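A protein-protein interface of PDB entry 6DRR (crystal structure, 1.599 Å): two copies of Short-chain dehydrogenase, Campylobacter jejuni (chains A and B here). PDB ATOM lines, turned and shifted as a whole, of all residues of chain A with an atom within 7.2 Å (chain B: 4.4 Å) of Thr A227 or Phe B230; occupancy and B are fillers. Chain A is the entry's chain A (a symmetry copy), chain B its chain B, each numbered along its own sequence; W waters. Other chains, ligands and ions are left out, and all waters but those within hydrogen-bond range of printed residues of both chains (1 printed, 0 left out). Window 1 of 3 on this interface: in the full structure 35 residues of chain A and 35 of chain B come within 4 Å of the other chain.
Among the printed residues, merely in contact across the chains: Met A1 with Leu B3, Leu A3 with Met B1, Asn A226 with Met B1, Asn A226 with Phe B230, Thr A227 with Phe B230, Phe A230 with Asn B226, Phe A230 with Thr B227 and Phe A230 with Phe B230.
O of Met B1 lies within hydrogen-bond range of N of Met A1, 2.8 Å away.
O of Leu B235 is in hydrogen-bond range of ND2 of Asn A226 (3.3 Å).
Asn A226 touches Met B1, but with the chains exchanged Met A1 does not touch Asn B226 (4.004 Å).
Asn A226 touches Phe B230, and with the chains exchanged Phe A230 touches Asn B226.
Thr A227 touches Phe B230, and with the chains exchanged Phe A230 touches Thr B227.
Phe A230 touches its own counterpart, Phe B230.
Water W1 lies within hydrogen-bond range of O of Glu A223 (2.6 Å), OG1 of Thr A227 (2.8 Å) and O of Leu B235 (2.8 Å).
Of the printed residues of chain B, Met A1 touches Met B1 (2.8 Å) and Leu B3 (3.97 Å).
Thr A227 touches just one residue of chain B: Phe B230 (3.6 Å).
Of the printed residues of chain A, Met B1 touches Met A1, Leu A3 and Asn A226.
Printed residues of chain A within 4 Å of Leu B3: Met A1 (3.97 Å).
Printed residues of chain A within 4 Å of Thr B227: Phe A230 (3.5 Å).
Ala B228 touches none of the printed residues of chain A.
Val B229 touches none of the printed residues of chain A.
Phe B230 touches three residues of chain A.
Of the printed residues of chain A, Leu B235 touches Asn A226 (3.3 Å).
The nearest printed residue of chain B that does not touch Thr A227 is Ala B236 (5.0 Å).
The nearest residue of chain A that does not touch Phe B230 is Met A1 (4.7 Å).
Printed residues of chain B that touch a printed residue of chain A: Met B1, Leu B3, Asn B226, Thr B227, Phe B230 and Leu B235.
Hydrophobic or aromatic side chains of chain B that line the printed part of chain A: Met B1, Leu B3, Phe B230 and Leu B235.
Of the 23 printed residues of chain A, 5 touch a printed residue of chain B.
Printed residues of chain A that touch a printed residue of chain B: Met A1, Leu A3, Asn A226, Thr A227 and Phe A230.
Hydrophobic or aromatic side chains of chain A that line the printed part of chain B: Met A1, Leu A3 and Phe A230.
Among the printed residues, no Asp or Glu carboxylate lies within 4 Å of a Lys or Arg side-chain nitrogen of the other chain.
The side-chain hydroxyl (OG1) of Thr B231 lies within hydrogen-bond range of the backbone carbonyl oxygen (O) of Thr B227.
The side-chain hydroxyl of Ser B233 is in hydrogen-bond range of the backbone carbonyl oxygen of Phe B230, 2.8 Å away.
OG of Ser B233 lies close to N of Leu B235 (3.0 Å).
O of Glu A222 sits close to ND2 of Asn A226 (3.3 Å).
The side-chain hydroxyl of Thr A231 sits at hydrogen-bond distance from the backbone carbonyl oxygen of Thr A227 (2.7 Å).
O of Phe A230 lies within hydrogen-bond range of OG of Ser A233 (2.8 Å).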
ATOM      1  N   MET A   1       6.993  22.850   4.091  1.00  0.00           N
ATOM      2  CA  MET A   1       6.863  22.611   5.528  1.00  0.00           C
ATOM      3  C   MET A   1       7.719  21.406   5.931  1.00  0.00           C
ATOM      4  O   MET A   1       7.504  20.293   5.449  1.00  0.00           O
ATOM      5  CB  MET A   1       5.391  22.392   5.898  1.00  0.00           C
ATOM      6  CG  MET A   1       5.142  22.044   7.349  1.00  0.00           C
ATOM      7  SD  MET A   1       3.375  21.863   7.738  1.00  0.00           S
ATOM      8  CE  MET A   1       3.033  23.485   8.420  1.00  0.00           C
ATOM      9  N   LEU A   3       8.526  18.644   8.269  1.00  0.00           N
ATOM     10  CA  LEU A   3       7.868  17.892   9.330  1.00  0.00           C
ATOM     11  C   LEU A   3       8.828  17.388  10.399  1.00  0.00           C
ATOM     12  O   LEU A   3       8.362  16.936  11.451  1.00  0.00           O
ATOM     13  CB  LEU A   3       7.104  16.709   8.728  1.00  0.00           C
ATOM     14  CG  LEU A   3       5.953  17.106   7.801  1.00  0.00           C
ATOM     15  CD1 LEU A   3       5.344  15.857   7.180  1.00  0.00           C
ATOM     16  CD2 LEU A   3       4.897  17.908   8.545  1.00  0.00           C
ATOM     17  N   LEU A  26       3.955   8.271   2.379  1.00  0.00           N
ATOM     18  CA  LEU A  26       4.169   9.670   2.737  1.00  0.00           C
ATOM     19  C   LEU A  26       5.198   9.801   3.851  1.00  0.00           C
ATOM     20  O   LEU A  26       6.053  10.692   3.809  1.00  0.00           O
ATOM     21  CB  LEU A  26       2.847  10.320   3.153  1.00  0.00           C
ATOM     22  CG  LEU A  26       2.931  11.783   3.593  1.00  0.00           C
ATOM     23  CD1 LEU A  26       3.499  12.659   2.488  1.00  0.00           C
ATOM     24  CD2 LEU A  26       1.551  12.277   4.000  1.00  0.00           C
ATOM     25  N   LEU A 136      -0.731   6.743  16.801  1.00  0.00           N
ATOM     26  CA  LEU A 136      -1.903   7.129  16.021  1.00  0.00           C
ATOM     27  C   LEU A 136      -2.786   5.913  15.802  1.00  0.00           C
ATOM     28  O   LEU A 136      -2.335   4.910  15.242  1.00  0.00           O
ATOM     29  CB  LEU A 136      -1.495   7.730  14.682  1.00  0.00           C
ATOM     30  CG  LEU A 136      -2.657   8.233  13.831  1.00  0.00           C
ATOM     31  CD1 LEU A 136      -3.359   9.408  14.535  1.00  0.00           C
ATOM     32  CD2 LEU A 136      -2.138   8.646  12.458  1.00  0.00           C
ATOM     33  N   ALA A 180      -6.176   9.877  17.199  1.00  0.00           N
ATOM     34  CA  ALA A 180      -6.878   8.962  16.313  1.00  0.00           C
ATOM     35  C   ALA A 180      -7.375   9.731  15.103  1.00  0.00           C
ATOM     36  O   ALA A 180      -7.632  10.935  15.182  1.00  0.00           O
ATOM     37  CB  ALA A 180      -8.061   8.285  17.016  1.00  0.00           C
ATOM     38  N   ILE A 181      -7.514   9.026  13.982  1.00  0.00           N
ATOM     39  CA  ILE A 181      -8.186   9.548  12.801  1.00  0.00           C
ATOM     40  C   ILE A 181      -9.399   8.669  12.518  1.00  0.00           C
ATOM     41  O   ILE A 181      -9.271   7.444  12.413  1.00  0.00           O
ATOM     42  CB  ILE A 181      -7.254   9.593  11.584  1.00  0.00           C
ATOM     43  CG1 ILE A 181      -6.177  10.661  11.788  1.00  0.00           C
ATOM     44  CG2 ILE A 181      -8.055   9.896  10.322  1.00  0.00           C
ATOM     45  CD1 ILE A 181      -5.241  10.740  10.627  1.00  0.00           C
ATOM     46  N   ILE A 221      -7.083   8.423  -0.158  1.00  0.00           N
ATOM     47  CA  ILE A 221      -6.035   7.896   0.703  1.00  0.00           C
ATOM     48  C   ILE A 221      -5.037   8.994   1.046  1.00  0.00           C
ATOM     49  O   ILE A 221      -4.580   9.101   2.192  1.00  0.00           O
ATOM     50  CB  ILE A 221      -5.351   6.693   0.024  1.00  0.00           C
ATOM     51  CG1 ILE A 221      -6.284   5.477   0.041  1.00  0.00           C
ATOM     52  CG2 ILE A 221      -4.007   6.384   0.712  1.00  0.00           C
ATOM     53  CD1 ILE A 221      -5.838   4.361  -0.914  1.00  0.00           C
ATOM     54  N   GLU A 222      -4.709   9.842   0.065  1.00  0.00           N
ATOM     55  CA  GLU A 222      -3.752  10.925   0.283  1.00  0.00           C
ATOM     56  C   GLU A 222      -4.238  11.882   1.362  1.00  0.00           C
ATOM     57  O   GLU A 222      -3.445  12.340   2.192  1.00  0.00           O
ATOM     58  CB  GLU A 222      -3.507  11.683  -1.023  1.00  0.00           C
ATOM     59  CG  GLU A 222      -2.708  10.914  -2.074  1.00  0.00           C
ATOM     60  CD  GLU A 222      -3.483   9.771  -2.739  1.00  0.00           C
ATOM     61  OE1 GLU A 222      -4.741   9.766  -2.737  1.00  0.00           O
ATOM     62  OE2 GLU A 222      -2.814   8.861  -3.274  1.00  0.00           O
ATOM     63  N   GLU A 223      -5.537  12.191   1.366  1.00  0.00           N
ATOM     64  CA  GLU A 223      -6.069  13.117   2.364  1.00  0.00           C
ATOM     65  C   GLU A 223      -5.956  12.540   3.767  1.00  0.00           C
ATOM     66  O   GLU A 223      -5.564  13.252   4.703  1.00  0.00           O
ATOM     67  CB  GLU A 223      -7.519  13.478   2.028  1.00  0.00           C
ATOM     68  CG  GLU A 223      -7.605  14.418   0.830  1.00  0.00           C
ATOM     69  CD  GLU A 223      -8.976  14.513   0.180  1.00  0.00           C
ATOM     70  OE1 GLU A 223      -9.781  13.567   0.282  1.00  0.00           O
ATOM     71  OE2 GLU A 223      -9.243  15.552  -0.472  1.00  0.00           O
ATOM     72  N   ILE A 224      -6.271  11.257   3.940  1.00  0.00           N
ATOM     73  CA  ILE A 224      -6.062  10.637   5.247  1.00  0.00           C
ATOM     74  C   ILE A 224      -4.586  10.679   5.618  1.00  0.00           C
ATOM     75  O   ILE A 224      -4.221  11.045   6.738  1.00  0.00           O
ATOM     76  CB  ILE A 224      -6.598   9.196   5.272  1.00  0.00           C
ATOM     77  CG1 ILE A 224      -8.092   9.164   4.926  1.00  0.00           C
ATOM     78  CG2 ILE A 224      -6.329   8.561   6.653  1.00  0.00           C
ATOM     79  CD1 ILE A 224      -8.954   9.985   5.887  1.00  0.00           C
ATOM     80  N   ALA A 225      -3.715  10.299   4.683  1.00  0.00           N
ATOM     81  CA  ALA A 225      -2.290  10.222   4.991  1.00  0.00           C
ATOM     82  C   ALA A 225      -1.715  11.585   5.351  1.00  0.00           C
ATOM     83  O   ALA A 225      -0.870  11.688   6.253  1.00  0.00           O
ATOM     84  CB  ALA A 225      -1.534   9.621   3.805  1.00  0.00           C
ATOM     85  N   ASN A 226      -2.149  12.638   4.653  1.00  0.00           N
ATOM     86  CA  ASN A 226      -1.624  13.972   4.929  1.00  0.00           C
ATOM     87  C   ASN A 226      -1.892  14.360   6.377  1.00  0.00           C
ATOM     88  O   ASN A 226      -0.985  14.792   7.093  1.00  0.00           O
ATOM     89  CB  ASN A 226      -2.241  15.004   3.976  1.00  0.00           C
ATOM     90  CG  ASN A 226      -1.710  14.896   2.551  1.00  0.00           C
ATOM     91  OD1 ASN A 226      -0.626  14.377   2.322  1.00  0.00           O
ATOM     92  ND2 ASN A 226      -2.471  15.411   1.597  1.00  0.00           N
ATOM     93  N   THR A 227      -3.135  14.185   6.831  1.00  0.00           N
ATOM     94  CA  THR A 227      -3.461  14.521   8.212  1.00  0.00           C
ATOM     95  C   THR A 227      -2.780  13.565   9.194  1.00  0.00           C
ATOM     96  O   THR A 227      -2.336  13.996  10.266  1.00  0.00           O
ATOM     97  CB  THR A 227      -4.981  14.532   8.398  1.00  0.00           C
ATOM     98  OG1 THR A 227      -5.516  15.705   7.773  1.00  0.00           O
ATOM     99  CG2 THR A 227      -5.357  14.558   9.891  1.00  0.00           C
ATOM    100  N   ALA A 228      -2.647  12.282   8.829  1.00  0.00           N
ATOM    101  CA  ALA A 228      -1.979  11.320   9.702  1.00  0.00           C
ATOM    102  C   ALA A 228      -0.525  11.702   9.940  1.00  0.00           C
ATOM    103  O   ALA A 228      -0.060  11.745  11.088  1.00  0.00           O
ATOM    104  CB  ALA A 228      -2.067   9.911   9.108  1.00  0.00           C
ATOM    105  N   VAL A 229       0.209  11.987   8.865  1.00  0.00           N
ATOM    106  CA  VAL A 229       1.634  12.236   9.011  1.00  0.00           C
ATOM    107  C   VAL A 229       1.883  13.592   9.663  1.00  0.00           C
ATOM    108  O   VAL A 229       2.779  13.727  10.509  1.00  0.00           O
ATOM    109  CB  VAL A 229       2.322  12.091   7.640  1.00  0.00           C
ATOM    110  CG1 VAL A 229       3.775  12.550   7.707  1.00  0.00           C
ATOM    111  CG2 VAL A 229       2.239  10.624   7.205  1.00  0.00           C
ATOM    112  N   PHE A 230       1.085  14.611   9.322  1.00  0.00           N
ATOM    113  CA  PHE A 230       1.192  15.878  10.041  1.00  0.00           C
ATOM    114  C   PHE A 230       0.971  15.674  11.539  1.00  0.00           C
ATOM    115  O   PHE A 230       1.729  16.192  12.367  1.00  0.00           O
ATOM    116  CB  PHE A 230       0.200  16.914   9.500  1.00  0.00           C
ATOM    117  CG  PHE A 230       0.195  18.191  10.294  1.00  0.00           C
ATOM    118  CD1 PHE A 230       1.148  19.175  10.048  1.00  0.00           C
ATOM    119  CD2 PHE A 230      -0.713  18.377  11.331  1.00  0.00           C
ATOM    120  CE1 PHE A 230       1.184  20.348  10.807  1.00  0.00           C
ATOM    121  CE2 PHE A 230      -0.695  19.560  12.093  1.00  0.00           C
ATOM    122  CZ  PHE A 230       0.252  20.542  11.826  1.00  0.00           C
ATOM    123  N   THR A 231      -0.060  14.909  11.902  1.00  0.00           N
ATOM    124  CA  THR A 231      -0.384  14.709  13.312  1.00  0.00           C
ATOM    125  C   THR A 231       0.708  13.935  14.046  1.00  0.00           C
ATOM    126  O   THR A 231       1.008  14.231  15.212  1.00  0.00           O
ATOM    127  CB  THR A 231      -1.730  13.999  13.427  1.00  0.00           C
ATOM    128  OG1 THR A 231      -2.735  14.808  12.808  1.00  0.00           O
ATOM    129  CG2 THR A 231      -2.103  13.767  14.903  1.00  0.00           C
ATOM    130  N   LEU A 232       1.309  12.936  13.384  1.00  0.00           N
ATOM    131  CA  LEU A 232       2.399  12.184  14.004  1.00  0.00           C
ATOM    132  C   LEU A 232       3.619  13.058  14.240  1.00  0.00           C
ATOM    133  O   LEU A 232       4.368  12.841  15.203  1.00  0.00           O
ATOM    134  CB  LEU A 232       2.798  10.998  13.118  1.00  0.00           C
ATOM    135  CG  LEU A 232       1.857   9.803  13.064  1.00  0.00           C
ATOM    136  CD1 LEU A 232       2.235   8.909  11.875  1.00  0.00           C
ATOM    137  CD2 LEU A 232       1.921   9.043  14.401  1.00  0.00           C
ATOM    138  N   SER A 233       3.846  14.026  13.362  1.00  0.00           N
ATOM    139  CA  SER A 233       5.080  14.780  13.351  1.00  0.00           C
ATOM    140  C   SER A 233       5.186  15.705  14.556  1.00  0.00           C
ATOM    141  O   SER A 233       4.184  16.060  15.186  1.00  0.00           O
ATOM    142  CB  SER A 233       5.172  15.615  12.077  1.00  0.00           C
ATOM    143  OG  SER A 233       4.427  16.815  12.235  1.00  0.00           O
ATOM    144  N   ALA A 236       2.877  18.884  15.250  1.00  0.00           N
ATOM    145  CA  ALA A 236       1.635  18.791  16.014  1.00  0.00           C
ATOM    146  C   ALA A 236       1.928  18.506  17.483  1.00  0.00           C
ATOM    147  O   ALA A 236       1.261  17.691  18.133  1.00  0.00           O
ATOM    148  CB  ALA A 236       0.725  17.720  15.417  1.00  0.00           C
ATOM    149  N   LEU A 244      -9.705  12.876  15.142  1.00  0.00           N
ATOM    150  CA  LEU A 244      -9.679  13.793  14.008  1.00  0.00           C
ATOM    151  C   LEU A 244     -10.543  13.254  12.880  1.00  0.00           C
ATOM    152  O   LEU A 244     -10.471  12.066  12.555  1.00  0.00           O
ATOM    153  CB  LEU A 244      -8.247  13.999  13.515  1.00  0.00           C
ATOM    154  CG  LEU A 244      -7.260  14.518  14.553  1.00  0.00           C
ATOM    155  CD1 LEU A 244      -5.847  14.511  13.965  1.00  0.00           C
ATOM    156  CD2 LEU A 244      -7.653  15.937  15.019  1.00  0.00           C
ATOM    157  N   MET A 245     -11.361  14.128  12.290  1.00  0.00           N
ATOM    158  CA  MET A 245     -12.267  13.754  11.205  1.00  0.00           C
ATOM    159  C   MET A 245     -11.956  14.538   9.943  1.00  0.00           C
ATOM    160  O   MET A 245     -12.525  15.618   9.723  1.00  0.00           O
ATOM    161  CB  MET A 245     -13.732  13.949  11.581  1.00  0.00           C
ATOM    162  CG  MET A 245     -14.274  12.888  12.471  1.00  0.00           C
ATOM    163  SD  MET A 245     -13.667  13.167  14.110  1.00  0.00           S
ATOM    164  CE  MET A 245     -15.187  13.486  14.984  1.00  0.00           C
ATOM    165  N   PRO A 246     -11.059  14.035   9.097  1.00  0.00           N
ATOM    166  CA  PRO A 246     -10.968  14.531   7.723  1.00  0.00           C
ATOM    167  C   PRO A 246     -11.901  13.689   6.879  1.00  0.00           C
ATOM    168  O   PRO A 246     -11.502  12.641   6.354  1.00  0.00           O
ATOM    169  CB  PRO A 246      -9.492  14.312   7.362  1.00  0.00           C
ATOM    170  CG  PRO A 246      -9.038  13.180   8.296  1.00  0.00           C
ATOM    171  CD  PRO A 246     -10.071  12.978   9.371  1.00  0.00           C
ATOM    172  N   MET B   1       7.161  18.563   3.258  1.00  0.00           N
ATOM    173  CA  MET B   1       5.752  18.574   2.879  1.00  0.00           C
ATOM    174  C   MET B   1       5.407  19.870   2.130  1.00  0.00           C
ATOM    175  O   MET B   1       5.537  20.966   2.678  1.00  0.00           O
ATOM    176  CB  MET B   1       4.872  18.398   4.123  1.00  0.00           C
ATOM    177  CG  MET B   1       3.391  18.353   3.834  1.00  0.00           C
ATOM    178  SD  MET B   1       2.362  17.980   5.280  1.00  0.00           S
ATOM    179  CE  MET B   1       2.110  16.216   5.082  1.00  0.00           C
ATOM    180  N   LEU B   3       2.883  22.324   0.889  1.00  0.00           N
ATOM    181  CA  LEU B   3       1.513  22.700   1.210  1.00  0.00           C
ATOM    182  C   LEU B   3       0.744  23.255   0.020  1.00  0.00           C
ATOM    183  O   LEU B   3      -0.473  23.431   0.127  1.00  0.00           O
ATOM    184  CB  LEU B   3       1.499  23.729   2.343  1.00  0.00           C
ATOM    185  CG  LEU B   3       2.048  23.244   3.689  1.00  0.00           C
ATOM    186  CD1 LEU B   3       2.015  24.393   4.693  1.00  0.00           C
ATOM    187  CD2 LEU B   3       1.281  22.017   4.198  1.00  0.00           C
ATOM    188  N   ASN B 226       1.062  26.040  13.007  1.00  0.00           N
ATOM    189  CA  ASN B 226       1.301  24.858  12.177  1.00  0.00           C
ATOM    190  C   ASN B 226      -0.008  24.169  11.833  1.00  0.00           C
ATOM    191  O   ASN B 226      -0.262  23.830  10.669  1.00  0.00           O
ATOM    192  CB  ASN B 226       2.224  23.872  12.890  1.00  0.00           C
ATOM    193  CG  ASN B 226       3.657  24.363  13.000  1.00  0.00           C
ATOM    194  OD1 ASN B 226       4.097  25.193  12.224  1.00  0.00           O
ATOM    195  ND2 ASN B 226       4.388  23.829  13.969  1.00  0.00           N
ATOM    196  N   THR B 227      -0.866  23.965  12.835  1.00  0.00           N
ATOM    197  CA  THR B 227      -2.145  23.324  12.549  1.00  0.00           C
ATOM    198  C   THR B 227      -3.037  24.234  11.716  1.00  0.00           C
ATOM    199  O   THR B 227      -3.741  23.760  10.818  1.00  0.00           O
ATOM    200  CB  THR B 227      -2.825  22.899  13.855  1.00  0.00           C
ATOM    201  OG1 THR B 227      -2.124  21.777  14.396  1.00  0.00           O
ATOM    202  CG2 THR B 227      -4.277  22.474  13.621  1.00  0.00           C
ATOM    203  N   ALA B 228      -2.983  25.550  11.954  1.00  0.00           N
ATOM    204  CA  ALA B 228      -3.788  26.484  11.169  1.00  0.00           C
ATOM    205  C   ALA B 228      -3.417  26.431   9.690  1.00  0.00           C
ATOM    206  O   ALA B 228      -4.288  26.284   8.822  1.00  0.00           O
ATOM    207  CB  ALA B 228      -3.622  27.908  11.711  1.00  0.00           C
ATOM    208  N   VAL B 229      -2.129  26.567   9.388  1.00  0.00           N
ATOM    209  CA  VAL B 229      -1.713  26.663   7.993  1.00  0.00           C
ATOM    210  C   VAL B 229      -1.886  25.323   7.287  1.00  0.00           C
ATOM    211  O   VAL B 229      -2.313  25.267   6.125  1.00  0.00           O
ATOM    212  CB  VAL B 229      -0.268  27.195   7.912  1.00  0.00           C
ATOM    213  CG1 VAL B 229       0.263  27.110   6.478  1.00  0.00           C
ATOM    214  CG2 VAL B 229      -0.232  28.643   8.407  1.00  0.00           C
ATOM    215  N   PHE B 230      -1.595  24.215   7.973  1.00  0.00           N
ATOM    216  CA  PHE B 230      -1.886  22.917   7.372  1.00  0.00           C
ATOM    217  C   PHE B 230      -3.368  22.791   7.032  1.00  0.00           C
ATOM    218  O   PHE B 230      -3.729  22.337   5.936  1.00  0.00           O
ATOM    219  CB  PHE B 230      -1.447  21.774   8.295  1.00  0.00           C
ATOM    220  CG  PHE B 230      -1.864  20.417   7.791  1.00  0.00           C
ATOM    221  CD1 PHE B 230      -1.073  19.735   6.875  1.00  0.00           C
ATOM    222  CD2 PHE B 230      -3.054  19.844   8.202  1.00  0.00           C
ATOM    223  CE1 PHE B 230      -1.453  18.499   6.392  1.00  0.00           C
ATOM    224  CE2 PHE B 230      -3.447  18.612   7.716  1.00  0.00           C
ATOM    225  CZ  PHE B 230      -2.639  17.934   6.813  1.00  0.00           C
ATOM    226  N   THR B 231      -4.245  23.202   7.955  1.00  0.00           N
ATOM    227  CA  THR B 231      -5.685  23.075   7.742  1.00  0.00           C
ATOM    228  C   THR B 231      -6.166  23.976   6.608  1.00  0.00           C
ATOM    229  O   THR B 231      -7.040  23.582   5.821  1.00  0.00           O
ATOM    230  CB  THR B 231      -6.409  23.405   9.047  1.00  0.00           C
ATOM    231  OG1 THR B 231      -5.997  22.468  10.057  1.00  0.00           O
ATOM    232  CG2 THR B 231      -7.935  23.339   8.874  1.00  0.00           C
ATOM    233  N   LEU B 232      -5.617  25.193   6.518  1.00  0.00           N
ATOM    234  CA  LEU B 232      -5.956  26.086   5.412  1.00  0.00           C
ATOM    235  C   LEU B 232      -5.553  25.499   4.065  1.00  0.00           C
ATOM    236  O   LEU B 232      -6.238  25.738   3.061  1.00  0.00           O
ATOM    237  CB  LEU B 232      -5.272  27.445   5.602  1.00  0.00           C
ATOM    238  CG  LEU B 232      -5.861  28.349   6.694  1.00  0.00           C
ATOM    239  CD1 LEU B 232      -4.889  29.472   7.042  1.00  0.00           C
ATOM    240  CD2 LEU B 232      -7.202  28.898   6.229  1.00  0.00           C
ATOM    241  N   SER B 233      -4.444  24.753   4.021  1.00  0.00           N
ATOM    242  CA  SER B 233      -3.815  24.359   2.773  1.00  0.00           C
ATOM    243  C   SER B 233      -4.634  23.306   2.034  1.00  0.00           C
ATOM    244  O   SER B 233      -5.465  22.620   2.626  1.00  0.00           O
ATOM    245  CB  SER B 233      -2.422  23.794   3.042  1.00  0.00           C
ATOM    246  OG  SER B 233      -2.514  22.432   3.427  1.00  0.00           O
ATOM    247  N   LEU B 235      -3.726  20.497   1.405  1.00  0.00           N
ATOM    248  CA  LEU B 235      -3.435  19.162   1.907  1.00  0.00           C
ATOM    249  C   LEU B 235      -4.514  18.667   2.855  1.00  0.00           C
ATOM    250  O   LEU B 235      -4.605  17.458   3.085  1.00  0.00           O
ATOM    251  CB  LEU B 235      -2.075  19.129   2.603  1.00  0.00           C
ATOM    252  CG  LEU B 235      -0.869  19.444   1.706  1.00  0.00           C
ATOM    253  CD1 LEU B 235       0.392  18.904   2.307  1.00  0.00           C
ATOM    254  CD2 LEU B 235      -1.062  18.899   0.313  1.00  0.00           C
ATOM    255  N   ALA B 236      -5.316  19.569   3.410  1.00  0.00           N
ATOM    256  CA  ALA B 236      -6.466  19.202   4.240  1.00  0.00           C
ATOM    257  C   ALA B 236      -7.756  19.307   3.438  1.00  0.00           C
ATOM    258  O   ALA B 236      -8.768  19.818   3.913  1.00  0.00           O
ATOM    259  CB  ALA B 236      -6.520  20.076   5.493  1.00  0.00           C
HETATM  260  O   HOH W   1      -5.832  15.829   5.010  1.00  0.00           O
